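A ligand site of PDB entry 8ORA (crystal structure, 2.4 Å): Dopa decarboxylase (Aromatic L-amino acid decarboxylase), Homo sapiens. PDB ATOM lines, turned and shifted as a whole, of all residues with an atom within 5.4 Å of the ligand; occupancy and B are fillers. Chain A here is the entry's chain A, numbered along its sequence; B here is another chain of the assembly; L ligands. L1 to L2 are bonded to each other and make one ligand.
OD2 of Asp 271 lies within hydrogen-bond range of N1 of LIG L1, 2.8 Å away.
The side-chain hydroxyl (OG) of Ser 149 sits at hydrogen-bond distance from an oxygen (O3) of LIG L1 (2.7 Å).
The side-chain hydroxyl (OG1) of Thr 246 sits at hydrogen-bond distance from an oxygen (O1) of LIG L1 (2.5 Å).
An oxygen (O4) of LIG L1 lies within hydrogen-bond range of a ring nitrogen (NE2) of His 302, 3.2 Å away.
The side-chain hydroxyl of Thr 82 sits at hydrogen-bond distance from an oxygen (O1) of LG2 L2 (3.4 Å).
The backbone NH of Ala 148 sits at hydrogen-bond distance from an oxygen (O4) of LIG L1, at 3.0 Å.
An oxygen (O4) of LIG L1 sits at hydrogen-bond distance from the side-chain amide nitrogen (ND2) of Asn 300 (2.9 Å).
The side-chain amino group of Lys 303 sits close to a nitrogen (N1) of LG2 L2, 2.9 Å away.
An oxygen (O3) of LIG L1 is in hydrogen-bond range of the backbone NH (N) of Ser 149 (3.3 Å).
NE2 of His 192 lies within hydrogen-bond range of O3 of LG2 L2 (3.5 Å).
The side-chain hydroxyl of Ser 147 is in hydrogen-bond range of the side-chain carboxylate of Glu 150.
The guanidinium group of Arg 447 lies within hydrogen-bond range of the backbone carbonyl oxygen of Thr 246, 2.8 Å away.
The side-chain hydroxyl (OG) of Ser 147 lies close to the backbone NH (N) of Ser 149.
A ring nitrogen (ND1) of His 192 is in hydrogen-bond range of the backbone NH (N) of Ser 194.
The backbone carbonyl oxygen of Tyr 79 sits at hydrogen-bond distance from the guanidinium group of Arg 447 (3.1 Å).
The backbone NH (N) of Ala 273 is in hydrogen-bond range of the side-chain carboxylate (OD1) of Asp 271, 3.3 Å away.
The side-chain amide nitrogen of Asn 300 lies within hydrogen-bond range of a ring nitrogen (NE2) of His 302, 3.1 Å away.
The backbone carbonyl oxygen (O) of Asp 271 lies within hydrogen-bond range of the backbone NH (N) of Leu 243 (2.8 Å).
Merely in contact with the ligand: Trp 71 (3.8 Å), Tyr 79 (3.8 Å), Phe 80 (3.5 Å), Pro 81 (3.6 Å), Ser 147 (3.2 Å), Gly 244 (3.97 Å), Ala 273 (3.7 Å), Ile 101 of chain B (3.4 Å), Phe 103 of chain B (3.8 Å), Tyr 332 of chain B (3.8 Å), Leu 333 of chain B (3.2 Å), Leu 353 of chain B (3.8 Å) and Gly 354 of chain B (3.99 Å).
Hydrophobic or aromatic side chains that line the ligand: Trp 71, Tyr 79, Phe 80, Ala 148, His 192, Ala 273, His 302, Ile 101 of chain B, Phe 103 of chain B, Tyr 332 of chain B, Leu 333 of chain B and Leu 353 of chain B.
22 residues have an atom within 4 Å of the ligand: Trp 71, Tyr 79, Phe 80, Pro 81, Thr 82, Ser 147, Ala 148, Ser 149, His 192, Gly 244, Thr 246, Asp 271, Ala 273, Asn 300, His 302, Lys 303, Ile 101 of chain B, Phe 103 of chain B, Tyr 332 of chain B, Leu 333 of chain B, Leu 353 of chain B and Gly 354 of chain B.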
ATOM      1  N   TRP A  71       5.184 -31.542   0.140  1.00  0.00           N
ATOM      2  CA  TRP A  71       5.965 -30.330  -0.060  1.00  0.00           C
ATOM      3  C   TRP A  71       6.134 -30.000  -1.527  1.00  0.00           C
ATOM      4  O   TRP A  71       6.355 -28.839  -1.884  1.00  0.00           O
ATOM      5  CB  TRP A  71       7.347 -30.470   0.606  1.00  0.00           C
ATOM      6  CG  TRP A  71       7.356 -30.194   2.069  1.00  0.00           C
ATOM      7  CD1 TRP A  71       6.714 -30.908   3.045  1.00  0.00           C
ATOM      8  CD2 TRP A  71       8.059 -29.143   2.745  1.00  0.00           C
ATOM      9  NE1 TRP A  71       6.977 -30.357   4.280  1.00  0.00           N
ATOM     10  CE2 TRP A  71       7.803 -29.269   4.119  1.00  0.00           C
ATOM     11  CE3 TRP A  71       8.880 -28.095   2.303  1.00  0.00           C
ATOM     12  CZ2 TRP A  71       8.329 -28.402   5.063  1.00  0.00           C
ATOM     13  CZ3 TRP A  71       9.413 -27.235   3.243  1.00  0.00           C
ATOM     14  CH2 TRP A  71       9.134 -27.389   4.604  1.00  0.00           C
ATOM     15  N   TYR A  79       6.017 -22.215   4.209  1.00  0.00           N
ATOM     16  CA  TYR A  79       7.393 -22.067   4.649  1.00  0.00           C
ATOM     17  C   TYR A  79       8.299 -21.577   3.533  1.00  0.00           C
ATOM     18  O   TYR A  79       8.143 -20.467   3.028  1.00  0.00           O
ATOM     19  CB  TYR A  79       7.924 -23.388   5.202  1.00  0.00           C
ATOM     20  CG  TYR A  79       6.962 -24.132   6.109  1.00  0.00           C
ATOM     21  CD1 TYR A  79       6.678 -23.671   7.385  1.00  0.00           C
ATOM     22  CD2 TYR A  79       6.341 -25.297   5.674  1.00  0.00           C
ATOM     23  CE1 TYR A  79       5.808 -24.349   8.212  1.00  0.00           C
ATOM     24  CE2 TYR A  79       5.464 -25.978   6.495  1.00  0.00           C
ATOM     25  CZ  TYR A  79       5.201 -25.507   7.762  1.00  0.00           C
ATOM     26  OH  TYR A  79       4.328 -26.181   8.576  1.00  0.00           O
ATOM     27  N   PHE A  80       9.264 -22.404   3.152  1.00  0.00           N
ATOM     28  CA  PHE A  80      10.174 -22.163   2.053  1.00  0.00           C
ATOM     29  C   PHE A  80      10.299 -23.452   1.256  1.00  0.00           C
ATOM     30  O   PHE A  80      10.025 -24.535   1.782  1.00  0.00           O
ATOM     31  CB  PHE A  80      11.550 -21.702   2.552  1.00  0.00           C
ATOM     32  CG  PHE A  80      11.661 -20.215   2.723  1.00  0.00           C
ATOM     33  CD1 PHE A  80      11.060 -19.346   1.823  1.00  0.00           C
ATOM     34  CD2 PHE A  80      12.366 -19.676   3.796  1.00  0.00           C
ATOM     35  CE1 PHE A  80      11.161 -17.978   1.985  1.00  0.00           C
ATOM     36  CE2 PHE A  80      12.466 -18.308   3.957  1.00  0.00           C
ATOM     37  CZ  PHE A  80      11.860 -17.456   3.053  1.00  0.00           C
ATOM     38  N   PRO A  81      10.712 -23.372  -0.013  1.00  0.00           N
ATOM     39  CA  PRO A  81      10.847 -24.595  -0.812  1.00  0.00           C
ATOM     40  C   PRO A  81      11.890 -25.538  -0.227  1.00  0.00           C
ATOM     41  O   PRO A  81      12.841 -25.114   0.420  1.00  0.00           O
ATOM     42  CB  PRO A  81      11.273 -24.074  -2.186  1.00  0.00           C
ATOM     43  CG  PRO A  81      11.825 -22.717  -1.929  1.00  0.00           C
ATOM     44  CD  PRO A  81      11.013 -22.170  -0.799  1.00  0.00           C
ATOM     45  N   THR A  82      11.685 -26.826  -0.468  1.00  0.00           N
ATOM     46  CA  THR A  82      12.692 -27.843  -0.208  1.00  0.00           C
ATOM     47  C   THR A  82      13.014 -28.558  -1.512  1.00  0.00           C
ATOM     48  O   THR A  82      12.170 -28.638  -2.410  1.00  0.00           O
ATOM     49  CB  THR A  82      12.236 -28.838   0.875  1.00  0.00           C
ATOM     50  OG1 THR A  82      13.380 -29.580   1.358  1.00  0.00           O
ATOM     51  CG2 THR A  82      11.209 -29.813   0.329  1.00  0.00           C
ATOM     52  N   GLY A 146      24.825 -30.363   7.874  1.00  0.00           N
ATOM     53  CA  GLY A 146      23.531 -31.012   7.865  1.00  0.00           C
ATOM     54  C   GLY A 146      22.375 -30.037   7.788  1.00  0.00           C
ATOM     55  O   GLY A 146      21.313 -30.363   7.259  1.00  0.00           O
ATOM     56  N   SER A 147      22.554 -28.827   8.320  1.00  0.00           N
ATOM     57  CA  SER A 147      21.488 -27.838   8.337  1.00  0.00           C
ATOM     58  C   SER A 147      22.091 -26.456   8.524  1.00  0.00           C
ATOM     59  O   SER A 147      23.235 -26.319   8.976  1.00  0.00           O
ATOM     60  CB  SER A 147      20.473 -28.129   9.438  1.00  0.00           C
ATOM     61  OG  SER A 147      21.027 -27.833  10.715  1.00  0.00           O
ATOM     62  N   ALA A 148      21.321 -25.435   8.164  1.00  0.00           N
ATOM     63  CA  ALA A 148      21.734 -24.067   8.438  1.00  0.00           C
ATOM     64  C   ALA A 148      21.753 -23.784   9.932  1.00  0.00           C
ATOM     65  O   ALA A 148      22.557 -22.964  10.399  1.00  0.00           O
ATOM     66  CB  ALA A 148      20.812 -23.077   7.723  1.00  0.00           C
ATOM     67  N   SER A 149      20.883 -24.444  10.698  1.00  0.00           N
ATOM     68  CA  SER A 149      20.895 -24.292  12.155  1.00  0.00           C
ATOM     69  C   SER A 149      22.189 -24.828  12.743  1.00  0.00           C
ATOM     70  O   SER A 149      22.751 -24.235  13.666  1.00  0.00           O
ATOM     71  CB  SER A 149      19.694 -25.014  12.759  1.00  0.00           C
ATOM     72  OG  SER A 149      18.487 -24.592  12.151  1.00  0.00           O
ATOM     73  N   GLU A 150      22.682 -25.946  12.208  1.00  0.00           N
ATOM     74  CA  GLU A 150      23.968 -26.490  12.664  1.00  0.00           C
ATOM     75  C   GLU A 150      25.117 -25.585  12.251  1.00  0.00           C
ATOM     76  O   GLU A 150      26.065 -25.394  13.030  1.00  0.00           O
ATOM     77  CB  GLU A 150      24.154 -27.903  12.116  1.00  0.00           C
ATOM     78  CG  GLU A 150      23.290 -28.957  12.770  1.00  0.00           C
ATOM     79  CD  GLU A 150      23.187 -30.224  11.958  1.00  0.00           C
ATOM     80  OE1 GLU A 150      22.280 -30.313  11.108  1.00  0.00           O
ATOM     81  OE2 GLU A 150      24.020 -31.138  12.168  1.00  0.00           O
ATOM     82  N   HIS A 192      15.921 -16.212  12.236  1.00  0.00           N
ATOM     83  CA  HIS A 192      15.361 -17.535  12.443  1.00  0.00           C
ATOM     84  C   HIS A 192      15.592 -17.999  13.881  1.00  0.00           C
ATOM     85  O   HIS A 192      16.490 -17.517  14.574  1.00  0.00           O
ATOM     86  CB  HIS A 192      15.975 -18.537  11.458  1.00  0.00           C
ATOM     87  CG  HIS A 192      15.314 -19.882  11.456  1.00  0.00           C
ATOM     88  ND1 HIS A 192      15.757 -20.934  12.223  1.00  0.00           N
ATOM     89  CD2 HIS A 192      14.249 -20.351  10.763  1.00  0.00           C
ATOM     90  CE1 HIS A 192      14.994 -21.987  12.017  1.00  0.00           C
ATOM     91  NE2 HIS A 192      14.066 -21.658  11.129  1.00  0.00           N
ATOM     92  N   SER A 194      16.946 -20.503  14.864  1.00  0.00           N
ATOM     93  CA  SER A 194      18.218 -21.207  15.030  1.00  0.00           C
ATOM     94  C   SER A 194      19.251 -20.346  15.747  1.00  0.00           C
ATOM     95  O   SER A 194      20.137 -20.890  16.429  1.00  0.00           O
ATOM     96  CB  SER A 194      18.747 -21.653  13.672  1.00  0.00           C
ATOM     97  OG  SER A 194      18.699 -20.602  12.727  1.00  0.00           O
ATOM     98  N   THR A 242      21.141 -11.839   8.509  1.00  0.00           N
ATOM     99  CA  THR A 242      20.265 -12.706   7.743  1.00  0.00           C
ATOM    100  C   THR A 242      19.963 -12.088   6.381  1.00  0.00           C
ATOM    101  O   THR A 242      19.544 -10.933   6.296  1.00  0.00           O
ATOM    102  CB  THR A 242      18.958 -12.984   8.495  1.00  0.00           C
ATOM    103  OG1 THR A 242      19.261 -13.581   9.765  1.00  0.00           O
ATOM    104  CG2 THR A 242      18.068 -13.917   7.693  1.00  0.00           C
ATOM    105  N   LEU A 243      20.167 -12.866   5.322  1.00  0.00           N
ATOM    106  CA  LEU A 243      19.775 -12.506   3.971  1.00  0.00           C
ATOM    107  C   LEU A 243      18.595 -13.393   3.572  1.00  0.00           C
ATOM    108  O   LEU A 243      18.726 -14.610   3.540  1.00  0.00           O
ATOM    109  CB  LEU A 243      20.934 -12.666   2.985  1.00  0.00           C
ATOM    110  CG  LEU A 243      22.175 -11.803   3.234  1.00  0.00           C
ATOM    111  CD1 LEU A 243      23.240 -12.088   2.192  1.00  0.00           C
ATOM    112  CD2 LEU A 243      21.800 -10.323   3.232  1.00  0.00           C
ATOM    113  N   GLY A 244      17.460 -12.770   3.273  1.00  0.00           N
ATOM    114  CA  GLY A 244      16.256 -13.522   3.011  1.00  0.00           C
ATOM    115  C   GLY A 244      15.665 -14.077   4.285  1.00  0.00           C
ATOM    116  O   GLY A 244      15.761 -15.276   4.564  1.00  0.00           O
ATOM    117  N   THR A 245      15.043 -13.210   5.077  1.00  0.00           N
ATOM    118  CA  THR A 245      14.506 -13.610   6.365  1.00  0.00           C
ATOM    119  C   THR A 245      13.346 -14.591   6.203  1.00  0.00           C
ATOM    120  O   THR A 245      12.620 -14.569   5.203  1.00  0.00           O
ATOM    121  CB  THR A 245      14.040 -12.387   7.154  1.00  0.00           C
ATOM    122  OG1 THR A 245      13.173 -11.586   6.345  1.00  0.00           O
ATOM    123  CG2 THR A 245      15.234 -11.556   7.599  1.00  0.00           C
ATOM    124  N   THR A 246      13.198 -15.459   7.207  1.00  0.00           N
ATOM    125  CA  THR A 246      12.084 -16.405   7.217  1.00  0.00           C
ATOM    126  C   THR A 246      10.744 -15.689   7.184  1.00  0.00           C
ATOM    127  O   THR A 246       9.798 -16.163   6.534  1.00  0.00           O
ATOM    128  CB  THR A 246      12.195 -17.279   8.473  1.00  0.00           C
ATOM    129  OG1 THR A 246      13.319 -18.162   8.352  1.00  0.00           O
ATOM    130  CG2 THR A 246      10.934 -18.095   8.696  1.00  0.00           C
ATOM    131  N   ASP A 271      23.579 -15.681   7.384  1.00  0.00           N
ATOM    132  CA  ASP A 271      22.588 -16.729   7.195  1.00  0.00           C
ATOM    133  C   ASP A 271      21.721 -16.349   5.992  1.00  0.00           C
ATOM    134  O   ASP A 271      20.880 -15.450   6.092  1.00  0.00           O
ATOM    135  CB  ASP A 271      21.743 -16.911   8.454  1.00  0.00           C
ATOM    136  CG  ASP A 271      20.719 -18.039   8.335  1.00  0.00           C
ATOM    137  OD1 ASP A 271      20.705 -18.745   7.292  1.00  0.00           O
ATOM    138  OD2 ASP A 271      19.938 -18.228   9.281  1.00  0.00           O
ATOM    139  N   ALA A 273      19.986 -18.871   4.023  1.00  0.00           N
ATOM    140  CA  ALA A 273      19.581 -20.235   3.726  1.00  0.00           C
ATOM    141  C   ALA A 273      18.738 -20.318   2.460  1.00  0.00           C
ATOM    142  O   ALA A 273      18.998 -21.139   1.574  1.00  0.00           O
ATOM    143  CB  ALA A 273      18.809 -20.817   4.912  1.00  0.00           C
ATOM    144  N   TYR A 274      17.721 -19.460   2.345  1.00  0.00           N
ATOM    145  CA  TYR A 274      16.832 -19.502   1.194  1.00  0.00           C
ATOM    146  C   TYR A 274      17.327 -18.636   0.043  1.00  0.00           C
ATOM    147  O   TYR A 274      17.372 -19.090  -1.105  1.00  0.00           O
ATOM    148  CB  TYR A 274      15.414 -19.086   1.597  1.00  0.00           C
ATOM    149  CG  TYR A 274      14.523 -18.748   0.430  1.00  0.00           C
ATOM    150  CD1 TYR A 274      14.086 -19.728  -0.449  1.00  0.00           C
ATOM    151  CD2 TYR A 274      14.126 -17.434   0.191  1.00  0.00           C
ATOM    152  CE1 TYR A 274      13.284 -19.418  -1.522  1.00  0.00           C
ATOM    153  CE2 TYR A 274      13.318 -17.117  -0.878  1.00  0.00           C
ATOM    154  CZ  TYR A 274      12.891 -18.114  -1.735  1.00  0.00           C
ATOM    155  OH  TYR A 274      12.090 -17.804  -2.808  1.00  0.00           O
ATOM    156  N   ASN A 300      21.410 -22.775   2.087  1.00  0.00           N
ATOM    157  CA  ASN A 300      20.926 -24.145   1.995  1.00  0.00           C
ATOM    158  C   ASN A 300      20.624 -24.504   0.553  1.00  0.00           C
ATOM    159  O   ASN A 300      19.605 -24.059   0.000  1.00  0.00           O
ATOM    160  CB  ASN A 300      19.665 -24.325   2.857  1.00  0.00           C
ATOM    161  CG  ASN A 300      19.980 -24.363   4.339  1.00  0.00           C
ATOM    162  OD1 ASN A 300      21.121 -24.604   4.741  1.00  0.00           O
ATOM    163  ND2 ASN A 300      18.960 -24.151   5.162  1.00  0.00           N
ATOM    164  N   HIS A 302      19.550 -27.323  -0.143  1.00  0.00           N
ATOM    165  CA  HIS A 302      18.384 -28.179   0.016  1.00  0.00           C
ATOM    166  C   HIS A 302      17.092 -27.382   0.125  1.00  0.00           C
ATOM    167  O   HIS A 302      16.045 -27.955   0.437  1.00  0.00           O
ATOM    168  CB  HIS A 302      18.548 -29.112   1.226  1.00  0.00           C
ATOM    169  CG  HIS A 302      18.676 -28.408   2.543  1.00  0.00           C
ATOM    170  ND1 HIS A 302      19.646 -28.747   3.464  1.00  0.00           N
ATOM    171  CD2 HIS A 302      17.960 -27.413   3.102  1.00  0.00           C
ATOM    172  CE1 HIS A 302      19.527 -27.984   4.531  1.00  0.00           C
ATOM    173  NE2 HIS A 302      18.512 -27.153   4.336  1.00  0.00           N
ATOM    174  N   LYS A 303      17.145 -26.076  -0.131  1.00  0.00           N
ATOM    175  CA  LYS A 303      15.961 -25.240  -0.237  1.00  0.00           C
ATOM    176  C   LYS A 303      15.654 -24.884  -1.683  1.00  0.00           C
ATOM    177  O   LYS A 303      14.619 -25.286  -2.214  1.00  0.00           O
ATOM    178  CB  LYS A 303      16.146 -23.960   0.578  1.00  0.00           C
ATOM    179  CG  LYS A 303      15.774 -24.055   2.025  1.00  0.00           C
ATOM    180  CD  LYS A 303      16.045 -22.725   2.673  1.00  0.00           C
ATOM    181  CE  LYS A 303      15.076 -22.465   3.786  1.00  0.00           C
ATOM    182  NZ  LYS A 303      15.113 -23.585   4.762  1.00  0.00           N
ATOM    183  N   PHE A 309      17.608 -32.575   0.587  1.00  0.00           N
ATOM    184  CA  PHE A 309      18.035 -32.626   1.980  1.00  0.00           C
ATOM    185  C   PHE A 309      18.655 -33.982   2.289  1.00  0.00           C
ATOM    186  O   PHE A 309      18.113 -35.027   1.897  1.00  0.00           O
ATOM    187  CB  PHE A 309      16.827 -32.355   2.893  1.00  0.00           C
ATOM    188  CG  PHE A 309      17.174 -32.127   4.332  1.00  0.00           C
ATOM    189  CD1 PHE A 309      17.185 -33.185   5.229  1.00  0.00           C
ATOM    190  CD2 PHE A 309      17.482 -30.866   4.796  1.00  0.00           C
ATOM    191  CE1 PHE A 309      17.496 -32.979   6.569  1.00  0.00           C
ATOM    192  CE2 PHE A 309      17.797 -30.653   6.130  1.00  0.00           C
ATOM    193  CZ  PHE A 309      17.805 -31.707   7.013  1.00  0.00           C
ATOM    194  N   ARG A 447       1.822 -15.462   4.324  1.00  0.00           N
ATOM    195  CA  ARG A 447       2.971 -15.634   3.451  1.00  0.00           C
ATOM    196  C   ARG A 447       2.611 -16.530   2.273  1.00  0.00           C
ATOM    197  O   ARG A 447       1.888 -17.521   2.448  1.00  0.00           O
ATOM    198  CB  ARG A 447       4.158 -16.237   4.205  1.00  0.00           C
ATOM    199  CG  ARG A 447       4.470 -15.577   5.530  1.00  0.00           C
ATOM    200  CD  ARG A 447       5.408 -16.435   6.373  1.00  0.00           C
ATOM    201  NE  ARG A 447       6.743 -16.552   5.788  1.00  0.00           N
ATOM    202  CZ  ARG A 447       7.165 -17.575   5.064  1.00  0.00           C
ATOM    203  NH1 ARG A 447       6.371 -18.607   4.795  1.00  0.00           N
ATOM    204  NH2 ARG A 447       8.408 -17.573   4.585  1.00  0.00           N
ATOM    205  N   ILE B 101      10.162 -32.294   5.211  1.00  0.00           N
ATOM    206  CA  ILE B 101      11.042 -31.726   6.221  1.00  0.00           C
ATOM    207  C   ILE B 101      10.271 -31.671   7.534  1.00  0.00           C
ATOM    208  O   ILE B 101       9.723 -30.620   7.889  1.00  0.00           O
ATOM    209  CB  ILE B 101      11.574 -30.346   5.811  1.00  0.00           C
ATOM    210  CG1 ILE B 101      12.105 -30.387   4.368  1.00  0.00           C
ATOM    211  CG2 ILE B 101      12.664 -29.880   6.766  1.00  0.00           C
ATOM    212  CD1 ILE B 101      13.224 -31.386   4.161  1.00  0.00           C
ATOM    213  N   PHE B 103      10.068 -30.974  10.658  1.00  0.00           N
ATOM    214  CA  PHE B 103      10.380 -30.284  11.902  1.00  0.00           C
ATOM    215  C   PHE B 103       9.194 -30.286  12.851  1.00  0.00           C
ATOM    216  O   PHE B 103       9.375 -30.287  14.067  1.00  0.00           O
ATOM    217  CB  PHE B 103      10.844 -28.858  11.613  1.00  0.00           C
ATOM    218  CG  PHE B 103      10.096 -28.186  10.490  1.00  0.00           C
ATOM    219  CD1 PHE B 103       8.792 -27.758  10.653  1.00  0.00           C
ATOM    220  CD2 PHE B 103      10.719 -27.974   9.264  1.00  0.00           C
ATOM    221  CE1 PHE B 103       8.118 -27.140   9.618  1.00  0.00           C
ATOM    222  CE2 PHE B 103      10.051 -27.363   8.226  1.00  0.00           C
ATOM    223  CZ  PHE B 103       8.749 -26.939   8.402  1.00  0.00           C
ATOM    224  N   TYR B 332       5.745 -19.055  12.485  1.00  0.00           N
ATOM    225  CA  TYR B 332       5.877 -19.755  11.216  1.00  0.00           C
ATOM    226  C   TYR B 332       6.099 -21.250  11.396  1.00  0.00           C
ATOM    227  O   TYR B 332       5.999 -21.994  10.417  1.00  0.00           O
ATOM    228  CB  TYR B 332       7.008 -19.147  10.388  1.00  0.00           C
ATOM    229  CG  TYR B 332       8.311 -18.924  11.129  1.00  0.00           C
ATOM    230  CD1 TYR B 332       9.218 -19.955  11.305  1.00  0.00           C
ATOM    231  CD2 TYR B 332       8.645 -17.665  11.640  1.00  0.00           C
ATOM    232  CE1 TYR B 332      10.412 -19.760  11.974  1.00  0.00           C
ATOM    233  CE2 TYR B 332       9.833 -17.463  12.313  1.00  0.00           C
ATOM    234  CZ  TYR B 332      10.722 -18.515  12.470  1.00  0.00           C
ATOM    235  OH  TYR B 332      11.904 -18.315  13.136  1.00  0.00           O
ATOM    236  N   LEU B 333       6.382 -21.707  12.612  1.00  0.00           N
ATOM    237  CA  LEU B 333       6.527 -23.134  12.915  1.00  0.00           C
ATOM    238  C   LEU B 333       5.455 -23.609  13.887  1.00  0.00           C
ATOM    239  O   LEU B 333       5.654 -24.595  14.611  1.00  0.00           O
ATOM    240  CB  LEU B 333       7.929 -23.417  13.449  1.00  0.00           C
ATOM    241  CG  LEU B 333       9.035 -23.218  12.404  1.00  0.00           C
ATOM    242  CD1 LEU B 333      10.429 -23.319  12.989  1.00  0.00           C
ATOM    243  CD2 LEU B 333       8.853 -24.211  11.270  1.00  0.00           C
ATOM    244  N   PRO B 352      19.571 -29.843  15.007  1.00  0.00           N
ATOM    245  CA  PRO B 352      18.977 -29.185  13.840  1.00  0.00           C
ATOM    246  C   PRO B 352      17.482 -28.974  14.040  1.00  0.00           C
ATOM    247  O   PRO B 352      16.861 -29.466  14.984  1.00  0.00           O
ATOM    248  CB  PRO B 352      19.256 -30.154  12.698  1.00  0.00           C
ATOM    249  CG  PRO B 352      19.305 -31.485  13.360  1.00  0.00           C
ATOM    250  CD  PRO B 352      19.961 -31.238  14.684  1.00  0.00           C
ATOM    251  N   LEU B 353      16.901 -28.225  13.102  1.00  0.00           N
ATOM    252  CA  LEU B 353      15.461 -28.069  13.012  1.00  0.00           C
ATOM    253  C   LEU B 353      14.849 -29.013  11.990  1.00  0.00           C
ATOM    254  O   LEU B 353      13.864 -29.690  12.275  1.00  0.00           O
ATOM    255  CB  LEU B 353      15.098 -26.618  12.654  1.00  0.00           C
ATOM    256  CG  LEU B 353      13.596 -26.356  12.477  1.00  0.00           C
ATOM    257  CD1 LEU B 353      12.965 -25.972  13.810  1.00  0.00           C
ATOM    258  CD2 LEU B 353      13.335 -25.290  11.420  1.00  0.00           C
ATOM    259  N   GLY B 354      15.426 -29.070  10.791  1.00  0.00           N
ATOM    260  CA  GLY B 354      14.935 -29.947   9.761  1.00  0.00           C
ATOM    261  C   GLY B 354      15.355 -31.394   9.963  1.00  0.00           C
ATOM    262  O   GLY B 354      16.340 -31.700  10.634  1.00  0.00           O
HETATM  263  N1  LIG L   1      17.773 -19.846   8.377  1.00  0.00           N
HETATM  264  C1  LIG L   1      16.752 -19.307   7.697  1.00  0.00           C
HETATM  265  C2  LIG L   1      16.828 -17.985   7.258  1.00  0.00           C
HETATM  266  C3  LIG L   1      15.620 -20.077   7.429  1.00  0.00           C
HETATM  267  O1  LIG L   1      14.595 -19.520   6.734  1.00  0.00           O
HETATM  268  C4  LIG L   1      15.505 -21.394   7.847  1.00  0.00           C
HETATM  269  C5  LIG L   1      14.340 -22.132   7.544  1.00  0.00           C
HETATM  270  C6  LIG L   1      16.567 -21.952   8.550  1.00  0.00           C
HETATM  271  C7  LIG L   1      17.703 -21.174   8.812  1.00  0.00           C
HETATM  272  C8  LIG L   1      16.515 -23.269   8.993  1.00  0.00           C
HETATM  273  O2  LIG L   1      17.619 -24.001   8.449  1.00  0.00           O
HETATM  274  P1  LIG L   1      17.575 -25.604   8.392  1.00  0.00           P
HETATM  275  O3  LIG L   1      18.163 -26.008   9.825  1.00  0.00           O
HETATM  276  O4  LIG L   1      18.523 -26.037   7.352  1.00  0.00           O
HETATM  277  O5  LIG L   1      16.149 -26.032   8.313  1.00  0.00           O
HETATM  278  N1  LG2 L   2      13.304 -22.204   6.558  1.00  0.00           N
HETATM  279  C1  LG2 L   2      12.430 -24.949   6.215  1.00  0.00           C
HETATM  280  C2  LG2 L   2      13.402 -25.808   6.714  1.00  0.00           C
HETATM  281  C3  LG2 L   2      14.093 -26.612   5.808  1.00  0.00           C
HETATM  282  C4  LG2 L   2      13.806 -26.556   4.449  1.00  0.00           C
HETATM  283  C5  LG2 L   2      12.830 -25.704   3.956  1.00  0.00           C
HETATM  284  C6  LG2 L   2      11.696 -24.120   7.055  1.00  0.00           C
HETATM  285  C7  LG2 L   2      12.499 -22.928   7.577  1.00  0.00           C
HETATM  286  C8  LG2 L   2      11.514 -22.063   8.420  1.00  0.00           C
HETATM  287  C9  LG2 L   2      10.472 -20.798   6.559  1.00  0.00           C
HETATM  288  C10 LG2 L   2      12.150 -24.900   4.852  1.00  0.00           C
HETATM  289  O1  LG2 L   2      14.526 -27.383   3.636  1.00  0.00           O
HETATM  290  O2  LG2 L   2      15.056 -27.491   6.195  1.00  0.00           O
HETATM  291  O3  LG2 L   2      11.138 -22.744   9.613  1.00  0.00           O
HETATM  292  O4  LG2 L   2      10.314 -21.627   7.716  1.00  0.00           O
